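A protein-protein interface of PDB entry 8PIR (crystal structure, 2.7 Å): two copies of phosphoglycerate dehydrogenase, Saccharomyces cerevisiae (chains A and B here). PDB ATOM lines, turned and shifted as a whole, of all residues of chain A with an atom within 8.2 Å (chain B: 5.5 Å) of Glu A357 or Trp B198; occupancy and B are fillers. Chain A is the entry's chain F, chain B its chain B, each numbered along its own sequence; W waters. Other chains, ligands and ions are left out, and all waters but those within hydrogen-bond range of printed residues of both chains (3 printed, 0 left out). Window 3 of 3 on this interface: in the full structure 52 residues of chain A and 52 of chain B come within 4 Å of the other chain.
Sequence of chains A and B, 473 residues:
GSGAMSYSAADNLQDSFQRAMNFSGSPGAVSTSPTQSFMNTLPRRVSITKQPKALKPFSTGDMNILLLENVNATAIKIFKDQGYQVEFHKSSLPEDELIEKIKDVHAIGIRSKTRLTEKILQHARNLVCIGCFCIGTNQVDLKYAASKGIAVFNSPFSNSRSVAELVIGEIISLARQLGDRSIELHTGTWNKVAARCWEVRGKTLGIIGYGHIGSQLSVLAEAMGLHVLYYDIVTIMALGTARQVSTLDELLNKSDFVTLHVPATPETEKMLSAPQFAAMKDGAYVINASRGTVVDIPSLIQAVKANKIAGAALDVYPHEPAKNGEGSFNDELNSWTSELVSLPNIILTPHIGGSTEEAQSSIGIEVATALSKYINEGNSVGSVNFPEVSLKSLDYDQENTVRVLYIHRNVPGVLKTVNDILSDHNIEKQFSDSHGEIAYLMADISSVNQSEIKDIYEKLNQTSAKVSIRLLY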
ATOM      1  N   ASN A  72     -18.827  37.021 -17.037  1.00  0.00           N
ATOM      2  CA  ASN A  72     -18.708  35.546 -17.192  1.00  0.00           C
ATOM      3  C   ASN A  72     -17.554  35.194 -18.143  1.00  0.00           C
ATOM      4  O   ASN A  72     -17.271  35.984 -19.056  1.00  0.00           O
ATOM      5  CB  ASN A  72     -20.026  34.957 -17.691  1.00  0.00           C
ATOM      6  CG  ASN A  72     -20.107  33.462 -17.502  1.00  0.00           C
ATOM      7  OD1 ASN A  72     -19.569  32.701 -18.305  1.00  0.00           O
ATOM      8  ND2 ASN A  72     -20.816  33.038 -16.471  1.00  0.00           N
ATOM      9  N   ALA A  73     -16.999  33.988 -18.002  1.00  0.00           N
ATOM     10  CA  ALA A  73     -15.823  33.485 -18.753  1.00  0.00           C
ATOM     11  C   ALA A  73     -16.186  33.243 -20.223  1.00  0.00           C
ATOM     12  O   ALA A  73     -15.272  33.212 -21.056  1.00  0.00           O
ATOM     13  CB  ALA A  73     -15.296  32.225 -18.109  1.00  0.00           C
ATOM     14  N   THR A  74     -17.473  33.087 -20.539  1.00  0.00           N
ATOM     15  CA  THR A  74     -17.963  32.893 -21.929  1.00  0.00           C
ATOM     16  C   THR A  74     -17.627  34.137 -22.755  1.00  0.00           C
ATOM     17  O   THR A  74     -17.255  33.987 -23.940  1.00  0.00           O
ATOM     18  CB  THR A  74     -19.468  32.610 -21.957  1.00  0.00           C
ATOM     19  OG1 THR A  74     -20.119  33.656 -21.230  1.00  0.00           O
ATOM     20  CG2 THR A  74     -19.821  31.255 -21.386  1.00  0.00           C
ATOM     21  N   SER A 162     -34.689  31.793 -15.551  1.00  0.00           N
ATOM     22  CA  SER A 162     -34.185  31.775 -14.152  1.00  0.00           C
ATOM     23  C   SER A 162     -35.250  32.356 -13.213  1.00  0.00           C
ATOM     24  O   SER A 162     -35.468  31.761 -12.146  1.00  0.00           O
ATOM     25  CB  SER A 162     -32.875  32.507 -14.024  1.00  0.00           C
ATOM     26  OG  SER A 162     -31.812  31.766 -14.616  1.00  0.00           O
ATOM     27  N   GLU A 165     -38.569  29.771 -13.185  1.00  0.00           N
ATOM     28  CA  GLU A 165     -38.265  28.614 -12.299  1.00  0.00           C
ATOM     29  C   GLU A 165     -38.346  29.057 -10.834  1.00  0.00           C
ATOM     30  O   GLU A 165     -38.912  28.308 -10.012  1.00  0.00           O
ATOM     31  CB  GLU A 165     -36.878  28.047 -12.588  1.00  0.00           C
ATOM     32  CG  GLU A 165     -36.757  27.431 -13.962  1.00  0.00           C
ATOM     33  CD  GLU A 165     -35.518  26.570 -14.122  1.00  0.00           C
ATOM     34  OE1 GLU A 165     -34.635  26.631 -13.234  1.00  0.00           O
ATOM     35  OE2 GLU A 165     -35.433  25.865 -15.150  1.00  0.00           O
ATOM     36  N   LEU A 166     -37.771  30.208 -10.491  1.00  0.00           N
ATOM     37  CA  LEU A 166     -37.831  30.709  -9.098  1.00  0.00           C
ATOM     38  C   LEU A 166     -39.294  30.782  -8.658  1.00  0.00           C
ATOM     39  O   LEU A 166     -39.584  30.366  -7.530  1.00  0.00           O
ATOM     40  CB  LEU A 166     -37.160  32.075  -8.972  1.00  0.00           C
ATOM     41  CG  LEU A 166     -37.210  32.644  -7.558  1.00  0.00           C
ATOM     42  CD1 LEU A 166     -36.108  32.037  -6.702  1.00  0.00           C
ATOM     43  CD2 LEU A 166     -37.128  34.163  -7.574  1.00  0.00           C
ATOM     44  N   GLY A 354     -32.442  36.442 -11.416  1.00  0.00           N
ATOM     45  CA  GLY A 354     -31.606  36.073 -12.575  1.00  0.00           C
ATOM     46  C   GLY A 354     -30.268  35.481 -12.157  1.00  0.00           C
ATOM     47  O   GLY A 354     -29.376  35.363 -13.017  1.00  0.00           O
ATOM     48  N   SER A 355     -30.065  35.253 -10.860  1.00  0.00           N
ATOM     49  CA  SER A 355     -28.740  34.911 -10.284  1.00  0.00           C
ATOM     50  C   SER A 355     -28.495  33.406 -10.424  1.00  0.00           C
ATOM     51  O   SER A 355     -28.568  32.697  -9.401  1.00  0.00           O
ATOM     52  CB  SER A 355     -28.635  35.385  -8.858  1.00  0.00           C
ATOM     53  OG  SER A 355     -28.608  36.806  -8.812  1.00  0.00           O
ATOM     54  N   THR A 356     -28.306  32.937 -11.663  1.00  0.00           N
ATOM     55  CA  THR A 356     -27.899  31.546 -11.999  1.00  0.00           C
ATOM     56  C   THR A 356     -26.658  31.569 -12.893  1.00  0.00           C
ATOM     57  O   THR A 356     -26.453  32.585 -13.582  1.00  0.00           O
ATOM     58  CB  THR A 356     -29.021  30.774 -12.702  1.00  0.00           C
ATOM     59  OG1 THR A 356     -29.179  31.273 -14.030  1.00  0.00           O
ATOM     60  CG2 THR A 356     -30.327  30.838 -11.940  1.00  0.00           C
ATOM     61  N   GLU A 357     -25.917  30.457 -12.924  1.00  0.00           N
ATOM     62  CA  GLU A 357     -24.745  30.244 -13.815  1.00  0.00           C
ATOM     63  C   GLU A 357     -25.196  30.300 -15.280  1.00  0.00           C
ATOM     64  O   GLU A 357     -24.473  30.900 -16.117  1.00  0.00           O
ATOM     65  CB  GLU A 357     -24.091  28.888 -13.536  1.00  0.00           C
ATOM     66  CG  GLU A 357     -23.407  28.801 -12.189  1.00  0.00           C
ATOM     67  CD  GLU A 357     -22.049  29.464 -12.112  1.00  0.00           C
ATOM     68  OE1 GLU A 357     -21.578  29.976 -13.143  1.00  0.00           O
ATOM     69  OE2 GLU A 357     -21.491  29.499 -11.006  1.00  0.00           O
ATOM     70  N   GLU A 358     -26.339  29.682 -15.586  1.00  0.00           N
ATOM     71  CA  GLU A 358     -26.905  29.665 -16.961  1.00  0.00           C
ATOM     72  C   GLU A 358     -27.112  31.110 -17.432  1.00  0.00           C
ATOM     73  O   GLU A 358     -26.598  31.454 -18.500  1.00  0.00           O
ATOM     74  CB  GLU A 358     -28.207  28.864 -17.014  1.00  0.00           C
ATOM     75  CG  GLU A 358     -27.998  27.360 -16.986  1.00  0.00           C
ATOM     76  CD  GLU A 358     -27.601  26.797 -15.631  1.00  0.00           C
ATOM     77  OE1 GLU A 358     -27.793  27.493 -14.621  1.00  0.00           O
ATOM     78  OE2 GLU A 358     -27.205  25.618 -15.573  1.00  0.00           O
ATOM     79  N   ALA A 359     -27.790  31.937 -16.631  1.00  0.00           N
ATOM     80  CA  ALA A 359     -28.178  33.325 -16.982  1.00  0.00           C
ATOM     81  C   ALA A 359     -26.929  34.176 -17.229  1.00  0.00           C
ATOM     82  O   ALA A 359     -26.888  34.870 -18.254  1.00  0.00           O
ATOM     83  CB  ALA A 359     -29.027  33.922 -15.891  1.00  0.00           C
ATOM     84  N   GLN A 360     -25.954  34.123 -16.320  1.00  0.00           N
ATOM     85  CA  GLN A 360     -24.695  34.914 -16.407  1.00  0.00           C
ATOM     86  C   GLN A 360     -23.925  34.520 -17.675  1.00  0.00           C
ATOM     87  O   GLN A 360     -23.391  35.427 -18.359  1.00  0.00           O
ATOM     88  CB  GLN A 360     -23.833  34.700 -15.159  1.00  0.00           C
ATOM     89  CG  GLN A 360     -24.347  35.434 -13.929  1.00  0.00           C
ATOM     90  CD  GLN A 360     -24.475  36.918 -14.179  1.00  0.00           C
ATOM     91  OE1 GLN A 360     -23.490  37.632 -14.325  1.00  0.00           O
ATOM     92  NE2 GLN A 360     -25.704  37.381 -14.317  1.00  0.00           N
ATOM     93  N   SER A 361     -23.867  33.223 -17.984  1.00  0.00           N
ATOM     94  CA  SER A 361     -23.058  32.679 -19.108  1.00  0.00           C
ATOM     95  C   SER A 361     -23.690  33.098 -20.441  1.00  0.00           C
ATOM     96  O   SER A 361     -22.934  33.481 -21.362  1.00  0.00           O
ATOM     97  CB  SER A 361     -22.887  31.184 -19.006  1.00  0.00           C
ATOM     98  OG  SER A 361     -24.134  30.523 -19.121  1.00  0.00           O
ATOM     99  N   SER A 362     -25.021  33.169 -20.495  1.00  0.00           N
ATOM    100  CA  SER A 362     -25.776  33.509 -21.733  1.00  0.00           C
ATOM    101  C   SER A 362     -25.869  35.034 -21.905  1.00  0.00           C
ATOM    102  O   SER A 362     -25.902  35.482 -23.061  1.00  0.00           O
ATOM    103  CB  SER A 362     -27.125  32.836 -21.760  1.00  0.00           C
ATOM    104  OG  SER A 362     -27.940  33.306 -20.707  1.00  0.00           O
ATOM    105  N   ILE A 363     -25.744  35.795 -20.814  1.00  0.00           N
ATOM    106  CA  ILE A 363     -25.448  37.257 -20.838  1.00  0.00           C
ATOM    107  C   ILE A 363     -24.062  37.452 -21.462  1.00  0.00           C
ATOM    108  O   ILE A 363     -23.948  38.271 -22.394  1.00  0.00           O
ATOM    109  CB  ILE A 363     -25.545  37.875 -19.427  1.00  0.00           C
ATOM    110  CG1 ILE A 363     -27.002  38.055 -18.999  1.00  0.00           C
ATOM    111  CG2 ILE A 363     -24.782  39.185 -19.343  1.00  0.00           C
ATOM    112  CD1 ILE A 363     -27.177  38.574 -17.590  1.00  0.00           C
ATOM    113  N   GLY A 364     -23.069  36.686 -21.002  1.00  0.00           N
ATOM    114  CA  GLY A 364     -21.714  36.670 -21.584  1.00  0.00           C
ATOM    115  C   GLY A 364     -21.744  36.524 -23.098  1.00  0.00           C
ATOM    116  O   GLY A 364     -21.082  37.310 -23.787  1.00  0.00           O
ATOM    117  N   ALA B 175     -31.266  24.008  -5.848  1.00  0.00           N
ATOM    118  CA  ALA B 175     -30.570  24.522  -7.050  1.00  0.00           C
ATOM    119  C   ALA B 175     -30.184  25.988  -6.842  1.00  0.00           C
ATOM    120  O   ALA B 175     -29.165  26.412  -7.413  1.00  0.00           O
ATOM    121  CB  ALA B 175     -31.446  24.347  -8.265  1.00  0.00           C
ATOM    122  N   ARG B 176     -31.026  26.747  -6.136  1.00  0.00           N
ATOM    123  CA  ARG B 176     -30.974  28.231  -6.086  1.00  0.00           C
ATOM    124  C   ARG B 176     -30.612  28.687  -4.667  1.00  0.00           C
ATOM    125  O   ARG B 176     -30.465  29.908  -4.465  1.00  0.00           O
ATOM    126  CB  ARG B 176     -32.323  28.801  -6.536  1.00  0.00           C
ATOM    127  CG  ARG B 176     -32.676  28.503  -7.982  1.00  0.00           C
ATOM    128  CD  ARG B 176     -31.840  29.341  -8.927  1.00  0.00           C
ATOM    129  NE  ARG B 176     -32.301  30.722  -9.000  1.00  0.00           N
ATOM    130  CZ  ARG B 176     -33.219  31.159  -9.854  1.00  0.00           C
ATOM    131  NH1 ARG B 176     -33.826  30.315 -10.673  1.00  0.00           N
ATOM    132  NH2 ARG B 176     -33.552  32.435  -9.873  1.00  0.00           N
ATOM    133  N   ALA B 194     -24.835  34.058  -7.366  1.00  0.00           N
ATOM    134  CA  ALA B 194     -25.170  33.304  -8.600  1.00  0.00           C
ATOM    135  C   ALA B 194     -24.256  32.079  -8.740  1.00  0.00           C
ATOM    136  O   ALA B 194     -24.556  31.212  -9.596  1.00  0.00           O
ATOM    137  CB  ALA B 194     -25.044  34.201  -9.801  1.00  0.00           C
ATOM    138  N   ALA B 195     -23.201  32.047  -7.937  1.00  0.00           N
ATOM    139  CA  ALA B 195     -22.198  30.977  -8.025  1.00  0.00           C
ATOM    140  C   ALA B 195     -22.772  29.650  -7.571  1.00  0.00           C
ATOM    141  O   ALA B 195     -23.296  29.588  -6.457  1.00  0.00           O
ATOM    142  CB  ALA B 195     -21.044  31.357  -7.162  1.00  0.00           C
ATOM    143  N   ARG B 196     -22.628  28.630  -8.406  1.00  0.00           N
ATOM    144  CA  ARG B 196     -23.105  27.280  -8.059  1.00  0.00           C
ATOM    145  C   ARG B 196     -24.600  27.352  -7.817  1.00  0.00           C
ATOM    146  O   ARG B 196     -25.116  26.502  -7.096  1.00  0.00           O
ATOM    147  CB  ARG B 196     -22.261  26.680  -6.939  1.00  0.00           C
ATOM    148  N   CYS B 197     -25.248  28.362  -8.374  1.00  0.00           N
ATOM    149  CA  CYS B 197     -26.724  28.405  -8.330  1.00  0.00           C
ATOM    150  C   CYS B 197     -27.134  28.064  -9.754  1.00  0.00           C
ATOM    151  O   CYS B 197     -26.607  28.667 -10.674  1.00  0.00           O
ATOM    152  CB  CYS B 197     -27.255  29.713  -7.766  1.00  0.00           C
ATOM    153  SG  CYS B 197     -26.990  29.898  -5.988  1.00  0.00           S
ATOM    154  N   TRP B 198     -28.045  27.128  -9.921  1.00  0.00           N
ATOM    155  CA  TRP B 198     -28.305  26.608 -11.277  1.00  0.00           C
ATOM    156  C   TRP B 198     -29.760  26.617 -11.690  1.00  0.00           C
ATOM    157  O   TRP B 198     -30.623  26.689 -10.820  1.00  0.00           O
ATOM    158  CB  TRP B 198     -27.876  25.143 -11.297  1.00  0.00           C
ATOM    159  CG  TRP B 198     -26.584  24.812 -10.628  1.00  0.00           C
ATOM    160  CD1 TRP B 198     -26.411  24.319  -9.371  1.00  0.00           C
ATOM    161  CD2 TRP B 198     -25.279  24.902 -11.213  1.00  0.00           C
ATOM    162  NE1 TRP B 198     -25.081  24.122  -9.124  1.00  0.00           N
ATOM    163  CE2 TRP B 198     -24.365  24.468 -10.237  1.00  0.00           C
ATOM    164  CE3 TRP B 198     -24.798  25.318 -12.455  1.00  0.00           C
ATOM    165  CZ2 TRP B 198     -22.994  24.437 -10.469  1.00  0.00           C
ATOM    166  CZ3 TRP B 198     -23.444  25.291 -12.682  1.00  0.00           C
ATOM    167  CH2 TRP B 198     -22.556  24.859 -11.700  1.00  0.00           C
ATOM    168  N   GLU B 199     -29.995  26.554 -12.995  1.00  0.00           N
ATOM    169  CA  GLU B 199     -31.372  26.387 -13.500  1.00  0.00           C
ATOM    170  C   GLU B 199     -31.562  24.883 -13.587  1.00  0.00           C
ATOM    171  O   GLU B 199     -30.596  24.199 -13.892  1.00  0.00           O
ATOM    172  CB  GLU B 199     -31.510  26.922 -14.918  1.00  0.00           C
ATOM    173  CG  GLU B 199     -31.537  28.426 -15.031  1.00  0.00           C
ATOM    174  CD  GLU B 199     -31.630  28.879 -16.475  1.00  0.00           C
ATOM    175  OE1 GLU B 199     -31.929  28.034 -17.333  1.00  0.00           O
ATOM    176  OE2 GLU B 199     -31.380  30.062 -16.739  1.00  0.00           O
ATOM    177  N   VAL B 200     -32.756  24.402 -13.280  1.00  0.00           N
ATOM    178  CA  VAL B 200     -33.002  22.930 -13.327  1.00  0.00           C
ATOM    179  C   VAL B 200     -32.975  22.475 -14.793  1.00  0.00           C
ATOM    180  O   VAL B 200     -32.375  21.443 -15.070  1.00  0.00           O
ATOM    181  CB  VAL B 200     -34.293  22.532 -12.582  1.00  0.00           C
ATOM    182  CG1 VAL B 200     -34.279  23.044 -11.150  1.00  0.00           C
ATOM    183  CG2 VAL B 200     -35.557  22.991 -13.291  1.00  0.00           C
ATOM    184  N   LYS B 203     -30.561  19.811 -16.438  1.00  0.00           N
ATOM    185  CA  LYS B 203     -29.965  18.997 -15.347  1.00  0.00           C
ATOM    186  C   LYS B 203     -30.576  17.594 -15.388  1.00  0.00           C
ATOM    187  O   LYS B 203     -31.622  17.419 -16.040  1.00  0.00           O
ATOM    188  CB  LYS B 203     -30.183  19.663 -13.984  1.00  0.00           C
ATOM    189  CG  LYS B 203     -29.511  21.018 -13.814  1.00  0.00           C
ATOM    190  CD  LYS B 203     -28.003  20.954 -13.814  1.00  0.00           C
ATOM    191  CE  LYS B 203     -27.345  22.319 -13.812  1.00  0.00           C
ATOM    192  NZ  LYS B 203     -27.964  23.248 -14.787  1.00  0.00           N
ATOM    193  N   GLY B 283     -20.782  18.356  -6.322  1.00  0.00           N
ATOM    194  CA  GLY B 283     -21.783  19.437  -6.253  1.00  0.00           C
ATOM    195  C   GLY B 283     -23.184  18.954  -6.585  1.00  0.00           C
ATOM    196  O   GLY B 283     -24.051  19.814  -6.814  1.00  0.00           O
ATOM    197  N   TYR B 285     -26.863  16.750  -5.558  1.00  0.00           N
ATOM    198  CA  TYR B 285     -27.876  17.014  -4.500  1.00  0.00           C
ATOM    199  C   TYR B 285     -28.608  15.710  -4.166  1.00  0.00           C
ATOM    200  O   TYR B 285     -28.926  14.944  -5.100  1.00  0.00           O
ATOM    201  CB  TYR B 285     -28.862  18.106  -4.940  1.00  0.00           C
ATOM    202  CG  TYR B 285     -28.238  19.428  -5.325  1.00  0.00           C
ATOM    203  CD1 TYR B 285     -27.954  20.396  -4.375  1.00  0.00           C
ATOM    204  CD2 TYR B 285     -27.926  19.715  -6.641  1.00  0.00           C
ATOM    205  CE1 TYR B 285     -27.379  21.609  -4.721  1.00  0.00           C
ATOM    206  CE2 TYR B 285     -27.373  20.931  -7.008  1.00  0.00           C
ATOM    207  CZ  TYR B 285     -27.099  21.883  -6.046  1.00  0.00           C
ATOM    208  OH  TYR B 285     -26.540  23.074  -6.405  1.00  0.00           O
HETATM  209  O   HOH W   1     -32.307  32.506 -17.468  1.00  0.00           O
HETATM  210  O   HOH W   2     -30.324  32.204  -7.373  1.00  0.00           O
HETATM  211  O   HOH W   3     -33.583  27.516 -10.912  1.00  0.00           O
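No position is printed for both chains.
Hydrophobic or aromatic side chains of chain A within 4 Å of the printed part of chain B: Leu A166.
Along chain B the printed residues that touch a printed residue of chain A span positions 176 to 203.
Among the printed residues, Asp or Glu carboxylates within 4 Å of a Lys or Arg side-chain nitrogen of the other chain: Glu A358 with Lys B203 (2.6 Å).
Glu A165 touches Glu B199.
CB of Leu A166 touches NH2 of Arg B176 (3.7 Å).
Ser A355 touches Ala B194.
Thr A356 touches Arg B176.
Thr A356 touches Ala B194 (C to O, 3.9 Å).
Thr A356 touches Cys B197 (CA to O, 3.4 Å).
Thr A356 touches Glu B199 (OG1 to OE2, 3.7 Å).
CA of Ala B195 touches OE2 of Glu A357, 3.4 Å away.
Glu A357 touches Trp B198.
Glu A358 touches Trp B198 (OE1 to CA, 3.5 Å).
N of Glu A357 lies within hydrogen-bond range of O of Cys B197 (3.0 Å).
The side-chain carboxylate of Glu A358 is in hydrogen-bond range of the backbone NH of Glu B199 (2.9 Å).
N of Val B200 sits at hydrogen-bond distance from OE1 of Glu A165 (2.9 Å).
The backbone carbonyl oxygen of Ser A162 is in hydrogen-bond range of the guanidinium group of Arg B176 (2.6 Å).
OE2 of Glu A357 is in hydrogen-bond range of N of Arg B196, at 3.0 Å.
OE2 of Glu A358 is in salt-bridge range of NZ of Lys B203 (2.6 Å).
OG of Ser A162 lies within hydrogen-bond range of OE2 of Glu B199 (2.8 Å).
Of chain B, only Ala B194, Ala B195, Arg B196, Cys B197 and Trp B198 come within 4 Å of Glu A357.
Printed residues of chain B within 4 Å of Thr A356: Arg B176, Ala B194, Cys B197 and Glu B199.
Printed residues of chain A within 4 Å of Val B200: Glu A165 (2.9 Å).
Gln A360 touches none of the printed residues of chain B.
The nearest residue of chain A that does not touch Trp B198 is Thr A356 (4.3 Å).
Water W3 lies within hydrogen-bond range of OE1 of Glu A165 (2.7 Å), NH1 of Arg B176 (2.8 Å) and O of Trp B198 (3.1 Å).
Water W1 bridges the side-chain carboxylate (OE2) of Glu B199 and the side-chain hydroxyl (OG) of Ser A162.
Water W2 lies within hydrogen-bond range of O of Ser A355 (2.7 Å) and NE of Arg B176 (3.0 Å).
SG of Cys B197 sits at hydrogen-bond distance from O of Ala B195 (3.7 Å).
OG of Ser A361 lies within hydrogen-bond range of O of Glu A357, 3.0 Å away.
The indole nitrogen (NE1) of Trp B198 sits close to the side-chain hydroxyl (OH) of Tyr B285, 3.3 Å away.
The backbone carbonyl oxygen (O) of Glu A358 lies within hydrogen-bond range of the side-chain hydroxyl (OG) of Ser A362 (3.2 Å).
The side-chain hydroxyl (OG1) of Thr A356 lies within hydrogen-bond range of the backbone NH (N) of Ala A359.
OG1 of Thr A356 lies within hydrogen-bond range of OG of Ser A162 (2.7 Å).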
